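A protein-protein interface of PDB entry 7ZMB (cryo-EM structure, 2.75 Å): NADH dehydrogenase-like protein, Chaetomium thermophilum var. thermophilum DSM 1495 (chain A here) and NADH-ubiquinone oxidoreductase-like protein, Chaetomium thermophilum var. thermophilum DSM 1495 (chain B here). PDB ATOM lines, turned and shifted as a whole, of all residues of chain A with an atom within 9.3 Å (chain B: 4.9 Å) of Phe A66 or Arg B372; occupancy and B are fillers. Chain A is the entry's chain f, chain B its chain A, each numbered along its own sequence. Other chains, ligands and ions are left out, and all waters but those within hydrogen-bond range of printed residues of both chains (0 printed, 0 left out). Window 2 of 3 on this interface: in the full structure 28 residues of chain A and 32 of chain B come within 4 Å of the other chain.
NE of Arg A63 lies close to ND2 of Asn B371 (3.1 Å).
O of Asn B371 lies within hydrogen-bond range of N of Gly A67 (3.2 Å).
O of Gly A67 sits at hydrogen-bond distance from NH2 of Arg B372 (3.4 Å).
N of Lys A12 is in hydrogen-bond range of O of Arg A63 (2.8 Å).
OD2 of Asp B368 lies within salt-bridge range of NH1 of Arg B372, 3.4 Å away.
Among the printed residues, pairs that only touch across the chains: Glu A65 with Glu B347 (3.6 Å), Phe A66 with Asn B371 (3.5 Å), Phe A66 with Arg B372 (3.9 Å) and Phe A66 with Gly B374 (3.9 Å).
Of chain B, only Asn B371, Arg B372 and Gly B374 come within 4 Å of Phe A66.
Printed residues of chain A within 4 Å of Arg B372: Phe A66 (3.9 Å) and Gly A67 (3.4 Å).
Of the printed residues of chain A, Gly B374 touches Phe A66 (3.9 Å).
Of the printed residues of chain B, Arg A63 touches Asn B371 (3.1 Å).
Pro B644 touches none of the printed residues of chain A.
The nearest printed residue of chain A that does not touch Gly B374 is Glu A65 (4.7 Å).
Of the 10 printed residues of chain A, 4 touch a printed residue of chain B.
Printed residues of chain B that touch a printed residue of chain A: Glu B347, Asn B371, Arg B372 and Gly B374.
Among the printed residues, 7 pairs touch across the chains.
Among the printed residues, no Asp or Glu carboxylate lies within 4 Å of a Lys or Arg side-chain nitrogen of the other chain.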
ATOM      1  N   GLY A  10       8.855 -11.554  -5.712  1.00  0.00           N
ATOM      2  CA  GLY A  10       8.420 -11.915  -4.380  1.00  0.00           C
ATOM      3  C   GLY A  10       8.025 -10.724  -3.533  1.00  0.00           C
ATOM      4  O   GLY A  10       7.200 -10.849  -2.625  1.00  0.00           O
ATOM      5  N   VAL A  11       8.601  -9.560  -3.807  1.00  0.00           N
ATOM      6  CA  VAL A  11       8.221  -8.361  -3.071  1.00  0.00           C
ATOM      7  C   VAL A  11       6.883  -7.870  -3.606  1.00  0.00           C
ATOM      8  O   VAL A  11       6.731  -7.593  -4.800  1.00  0.00           O
ATOM      9  CB  VAL A  11       9.310  -7.278  -3.148  1.00  0.00           C
ATOM     10  CG1 VAL A  11      10.578  -7.785  -2.511  1.00  0.00           C
ATOM     11  CG2 VAL A  11       9.599  -6.909  -4.575  1.00  0.00           C
ATOM     12  N   LYS A  12       5.896  -7.798  -2.721  1.00  0.00           N
ATOM     13  CA  LYS A  12       4.544  -7.460  -3.117  1.00  0.00           C
ATOM     14  C   LYS A  12       4.202  -6.001  -2.856  1.00  0.00           C
ATOM     15  O   LYS A  12       3.295  -5.477  -3.505  1.00  0.00           O
ATOM     16  CB  LYS A  12       3.552  -8.371  -2.388  1.00  0.00           C
ATOM     17  CG  LYS A  12       3.825  -9.848  -2.650  1.00  0.00           C
ATOM     18  CD  LYS A  12       3.792 -10.180  -4.138  1.00  0.00           C
ATOM     19  CE  LYS A  12       2.378 -10.346  -4.650  1.00  0.00           C
ATOM     20  NZ  LYS A  12       1.541 -11.014  -3.623  1.00  0.00           N
ATOM     21  N   ARG A  63       6.619  -6.409   2.037  1.00  0.00           N
ATOM     22  CA  ARG A  63       5.675  -7.523   2.233  1.00  0.00           C
ATOM     23  C   ARG A  63       5.959  -8.583   1.174  1.00  0.00           C
ATOM     24  O   ARG A  63       6.039  -8.226  -0.008  1.00  0.00           O
ATOM     25  CB  ARG A  63       4.229  -7.032   2.256  1.00  0.00           C
ATOM     26  CG  ARG A  63       3.288  -7.972   2.993  1.00  0.00           C
ATOM     27  CD  ARG A  63       1.893  -7.392   3.095  1.00  0.00           C
ATOM     28  NE  ARG A  63       1.521  -6.583   1.944  1.00  0.00           N
ATOM     29  CZ  ARG A  63       1.315  -7.064   0.725  1.00  0.00           C
ATOM     30  NH1 ARG A  63       0.964  -6.257  -0.259  1.00  0.00           N
ATOM     31  NH2 ARG A  63       1.477  -8.353   0.494  1.00  0.00           N
ATOM     32  N   TYR A  64       6.129  -9.826   1.609  1.00  0.00           N
ATOM     33  CA  TYR A  64       6.433 -10.938   0.730  1.00  0.00           C
ATOM     34  C   TYR A  64       5.230 -11.870   0.634  1.00  0.00           C
ATOM     35  O   TYR A  64       4.189 -11.665   1.258  1.00  0.00           O
ATOM     36  CB  TYR A  64       7.675 -11.678   1.218  1.00  0.00           C
ATOM     37  CG  TYR A  64       8.881 -10.792   1.429  1.00  0.00           C
ATOM     38  CD1 TYR A  64       9.724 -10.477   0.376  1.00  0.00           C
ATOM     39  CD2 TYR A  64       9.186 -10.288   2.679  1.00  0.00           C
ATOM     40  CE1 TYR A  64      10.825  -9.677   0.561  1.00  0.00           C
ATOM     41  CE2 TYR A  64      10.285  -9.482   2.867  1.00  0.00           C
ATOM     42  CZ  TYR A  64      11.101  -9.184   1.803  1.00  0.00           C
ATOM     43  OH  TYR A  64      12.200  -8.385   1.980  1.00  0.00           O
ATOM     44  N   GLU A  65       5.400 -12.921  -0.150  1.00  0.00           N
ATOM     45  CA  GLU A  65       4.283 -13.731  -0.605  1.00  0.00           C
ATOM     46  C   GLU A  65       3.714 -14.537   0.563  1.00  0.00           C
ATOM     47  O   GLU A  65       4.432 -14.900   1.498  1.00  0.00           O
ATOM     48  CB  GLU A  65       4.779 -14.623  -1.744  1.00  0.00           C
ATOM     49  CG  GLU A  65       3.750 -15.202  -2.683  1.00  0.00           C
ATOM     50  CD  GLU A  65       3.145 -16.488  -2.212  1.00  0.00           C
ATOM     51  OE1 GLU A  65       3.772 -17.193  -1.395  1.00  0.00           O
ATOM     52  OE2 GLU A  65       2.061 -16.818  -2.729  1.00  0.00           O
ATOM     53  N   PHE A  66       2.404 -14.806   0.510  1.00  0.00           N
ATOM     54  CA  PHE A  66       1.670 -15.398   1.642  1.00  0.00           C
ATOM     55  C   PHE A  66       1.765 -14.556   2.911  1.00  0.00           C
ATOM     56  O   PHE A  66       1.895 -15.081   4.014  1.00  0.00           O
ATOM     57  CB  PHE A  66       2.105 -16.837   1.927  1.00  0.00           C
ATOM     58  CG  PHE A  66       1.672 -17.828   0.894  1.00  0.00           C
ATOM     59  CD1 PHE A  66       0.799 -17.467  -0.112  1.00  0.00           C
ATOM     60  CD2 PHE A  66       2.026 -19.161   1.016  1.00  0.00           C
ATOM     61  CE1 PHE A  66       0.364 -18.397  -1.032  1.00  0.00           C
ATOM     62  CE2 PHE A  66       1.605 -20.094   0.093  1.00  0.00           C
ATOM     63  CZ  PHE A  66       0.770 -19.711  -0.931  1.00  0.00           C
ATOM     64  N   GLY A  67       1.695 -13.241   2.756  1.00  0.00           N
ATOM     65  CA  GLY A  67       1.444 -12.363   3.875  1.00  0.00           C
ATOM     66  C   GLY A  67       2.635 -12.005   4.729  1.00  0.00           C
ATOM     67  O   GLY A  67       2.485 -11.190   5.646  1.00  0.00           O
ATOM     68  N   ARG A  68       3.810 -12.564   4.466  1.00  0.00           N
ATOM     69  CA  ARG A  68       4.951 -12.304   5.330  1.00  0.00           C
ATOM     70  C   ARG A  68       5.563 -10.944   5.034  1.00  0.00           C
ATOM     71  O   ARG A  68       5.502 -10.436   3.914  1.00  0.00           O
ATOM     72  CB  ARG A  68       5.998 -13.404   5.198  1.00  0.00           C
ATOM     73  CG  ARG A  68       6.551 -13.600   3.815  1.00  0.00           C
ATOM     74  CD  ARG A  68       7.576 -14.712   3.842  1.00  0.00           C
ATOM     75  NE  ARG A  68       8.749 -14.317   4.613  1.00  0.00           N
ATOM     76  CZ  ARG A  68       9.807 -13.706   4.093  1.00  0.00           C
ATOM     77  NH1 ARG A  68      10.834 -13.379   4.866  1.00  0.00           N
ATOM     78  NH2 ARG A  68       9.844 -13.437   2.798  1.00  0.00           N
ATOM     79  N   GLU A  69       6.148 -10.350   6.064  1.00  0.00           N
ATOM     80  CA  GLU A  69       6.572  -8.964   6.009  1.00  0.00           C
ATOM     81  C   GLU A  69       7.865  -8.805   6.796  1.00  0.00           C
ATOM     82  O   GLU A  69       8.056  -9.433   7.839  1.00  0.00           O
ATOM     83  CB  GLU A  69       5.464  -8.050   6.558  1.00  0.00           C
ATOM     84  CG  GLU A  69       5.696  -6.567   6.402  1.00  0.00           C
ATOM     85  CD  GLU A  69       4.394  -5.788   6.225  1.00  0.00           C
ATOM     86  OE1 GLU A  69       3.793  -5.375   7.238  1.00  0.00           O
ATOM     87  OE2 GLU A  69       3.978  -5.581   5.066  1.00  0.00           O
ATOM     88  N   GLU B 347      -3.176 -17.766  -6.459  1.00  0.00           N
ATOM     89  CA  GLU B 347      -2.977 -16.332  -6.350  1.00  0.00           C
ATOM     90  C   GLU B 347      -4.022 -15.582  -7.167  1.00  0.00           C
ATOM     91  O   GLU B 347      -4.171 -15.812  -8.371  1.00  0.00           O
ATOM     92  CB  GLU B 347      -1.573 -15.958  -6.820  1.00  0.00           C
ATOM     93  CG  GLU B 347      -0.459 -16.502  -5.939  1.00  0.00           C
ATOM     94  CD  GLU B 347      -0.123 -17.947  -6.259  1.00  0.00           C
ATOM     95  OE1 GLU B 347      -0.727 -18.504  -7.199  1.00  0.00           O
ATOM     96  OE2 GLU B 347       0.742 -18.527  -5.568  1.00  0.00           O
ATOM     97  N   ASP B 368      -4.981  -8.055   5.303  1.00  0.00           N
ATOM     98  CA  ASP B 368      -4.144  -9.054   5.954  1.00  0.00           C
ATOM     99  C   ASP B 368      -4.685 -10.466   5.773  1.00  0.00           C
ATOM    100  O   ASP B 368      -3.911 -11.424   5.788  1.00  0.00           O
ATOM    101  CB  ASP B 368      -3.999  -8.724   7.436  1.00  0.00           C
ATOM    102  CG  ASP B 368      -3.104  -7.532   7.675  1.00  0.00           C
ATOM    103  OD1 ASP B 368      -2.830  -6.800   6.708  1.00  0.00           O
ATOM    104  OD2 ASP B 368      -2.674  -7.324   8.827  1.00  0.00           O
ATOM    105  N   LEU B 369      -5.998 -10.624   5.604  1.00  0.00           N
ATOM    106  CA  LEU B 369      -6.544 -11.954   5.358  1.00  0.00           C
ATOM    107  C   LEU B 369      -6.259 -12.408   3.935  1.00  0.00           C
ATOM    108  O   LEU B 369      -5.785 -13.527   3.716  1.00  0.00           O
ATOM    109  CB  LEU B 369      -8.049 -11.979   5.617  1.00  0.00           C
ATOM    110  CG  LEU B 369      -8.751 -13.294   5.266  1.00  0.00           C
ATOM    111  CD1 LEU B 369      -8.030 -14.504   5.862  1.00  0.00           C
ATOM    112  CD2 LEU B 369     -10.209 -13.275   5.664  1.00  0.00           C
ATOM    113  N   ALA B 370      -6.546 -11.554   2.956  1.00  0.00           N
ATOM    114  CA  ALA B 370      -6.317 -11.925   1.565  1.00  0.00           C
ATOM    115  C   ALA B 370      -4.836 -12.122   1.278  1.00  0.00           C
ATOM    116  O   ALA B 370      -4.465 -13.025   0.524  1.00  0.00           O
ATOM    117  CB  ALA B 370      -6.911 -10.874   0.633  1.00  0.00           C
ATOM    118  N   ASN B 371      -3.977 -11.285   1.869  1.00  0.00           N
ATOM    119  CA  ASN B 371      -2.545 -11.397   1.610  1.00  0.00           C
ATOM    120  C   ASN B 371      -2.013 -12.758   2.033  1.00  0.00           C
ATOM    121  O   ASN B 371      -1.201 -13.362   1.325  1.00  0.00           O
ATOM    122  CB  ASN B 371      -1.785 -10.284   2.331  1.00  0.00           C
ATOM    123  CG  ASN B 371      -1.804  -8.972   1.575  1.00  0.00           C
ATOM    124  OD1 ASN B 371      -2.279  -8.898   0.450  1.00  0.00           O
ATOM    125  ND2 ASN B 371      -1.289  -7.929   2.198  1.00  0.00           N
ATOM    126  N   ARG B 372      -2.462 -13.264   3.178  1.00  0.00           N
ATOM    127  CA  ARG B 372      -2.017 -14.573   3.638  1.00  0.00           C
ATOM    128  C   ARG B 372      -2.743 -15.719   2.955  1.00  0.00           C
ATOM    129  O   ARG B 372      -2.298 -16.863   3.067  1.00  0.00           O
ATOM    130  CB  ARG B 372      -2.166 -14.671   5.155  1.00  0.00           C
ATOM    131  CG  ARG B 372      -1.589 -13.471   5.879  1.00  0.00           C
ATOM    132  CD  ARG B 372      -1.464 -13.740   7.359  1.00  0.00           C
ATOM    133  NE  ARG B 372      -1.970 -12.643   8.173  1.00  0.00           N
ATOM    134  CZ  ARG B 372      -1.295 -11.528   8.421  1.00  0.00           C
ATOM    135  NH1 ARG B 372      -1.834 -10.581   9.174  1.00  0.00           N
ATOM    136  NH2 ARG B 372      -0.077 -11.361   7.923  1.00  0.00           N
ATOM    137  N   LEU B 373      -3.840 -15.447   2.253  1.00  0.00           N
ATOM    138  CA  LEU B 373      -4.436 -16.454   1.394  1.00  0.00           C
ATOM    139  C   LEU B 373      -3.806 -16.485   0.011  1.00  0.00           C
ATOM    140  O   LEU B 373      -4.147 -17.362  -0.788  1.00  0.00           O
ATOM    141  CB  LEU B 373      -5.939 -16.223   1.260  1.00  0.00           C
ATOM    142  CG  LEU B 373      -6.752 -16.361   2.542  1.00  0.00           C
ATOM    143  CD1 LEU B 373      -8.081 -15.648   2.398  1.00  0.00           C
ATOM    144  CD2 LEU B 373      -6.955 -17.812   2.939  1.00  0.00           C
ATOM    145  N   GLY B 374      -2.905 -15.560  -0.292  1.00  0.00           N
ATOM    146  CA  GLY B 374      -2.257 -15.523  -1.581  1.00  0.00           C
ATOM    147  C   GLY B 374      -2.845 -14.556  -2.575  1.00  0.00           C
ATOM    148  O   GLY B 374      -2.422 -14.557  -3.735  1.00  0.00           O
ATOM    149  N   VAL B 641      -5.339 -19.433   8.497  1.00  0.00           N
ATOM    150  CA  VAL B 641      -4.334 -18.394   8.701  1.00  0.00           C
ATOM    151  C   VAL B 641      -4.842 -17.344   9.684  1.00  0.00           C
ATOM    152  O   VAL B 641      -5.218 -16.239   9.269  1.00  0.00           O
ATOM    153  CB  VAL B 641      -3.922 -17.767   7.360  1.00  0.00           C
ATOM    154  CG1 VAL B 641      -3.016 -18.714   6.605  1.00  0.00           C
ATOM    155  CG2 VAL B 641      -5.142 -17.483   6.512  1.00  0.00           C
ATOM    156  N   PRO B 642      -4.866 -17.632  10.983  1.00  0.00           N
ATOM    157  CA  PRO B 642      -5.311 -16.625  11.956  1.00  0.00           C
ATOM    158  C   PRO B 642      -4.438 -15.377  11.942  1.00  0.00           C
ATOM    159  O   PRO B 642      -3.221 -15.448  11.777  1.00  0.00           O
ATOM    160  CB  PRO B 642      -5.208 -17.362  13.292  1.00  0.00           C
ATOM    161  CG  PRO B 642      -4.269 -18.476  13.034  1.00  0.00           C
ATOM    162  CD  PRO B 642      -4.512 -18.896  11.634  1.00  0.00           C
ATOM    163  N   LEU B 643      -5.077 -14.229  12.117  1.00  0.00           N
ATOM    164  CA  LEU B 643      -4.466 -12.906  12.148  1.00  0.00           C
ATOM    165  C   LEU B 643      -4.020 -12.562  13.569  1.00  0.00           C
ATOM    166  O   LEU B 643      -4.740 -12.844  14.528  1.00  0.00           O
ATOM    167  CB  LEU B 643      -5.444 -11.855  11.640  1.00  0.00           C
ATOM    168  CG  LEU B 643      -6.050 -12.154  10.270  1.00  0.00           C
ATOM    169  CD1 LEU B 643      -7.291 -11.319  10.010  1.00  0.00           C
ATOM    170  CD2 LEU B 643      -5.036 -11.974   9.168  1.00  0.00           C
ATOM    171  N   PRO B 644      -2.835 -11.961  13.711  1.00  0.00           N
ATOM    172  CA  PRO B 644      -2.208 -11.876  15.046  1.00  0.00           C
ATOM    173  C   PRO B 644      -3.047 -11.180  16.104  1.00  0.00           C
ATOM    174  O   PRO B 644      -3.138 -11.653  17.242  1.00  0.00           O
ATOM    175  CB  PRO B 644      -0.912 -11.102  14.761  1.00  0.00           C
ATOM    176  CG  PRO B 644      -1.052 -10.566  13.371  1.00  0.00           C
ATOM    177  CD  PRO B 644      -1.937 -11.494  12.649  1.00  0.00           C
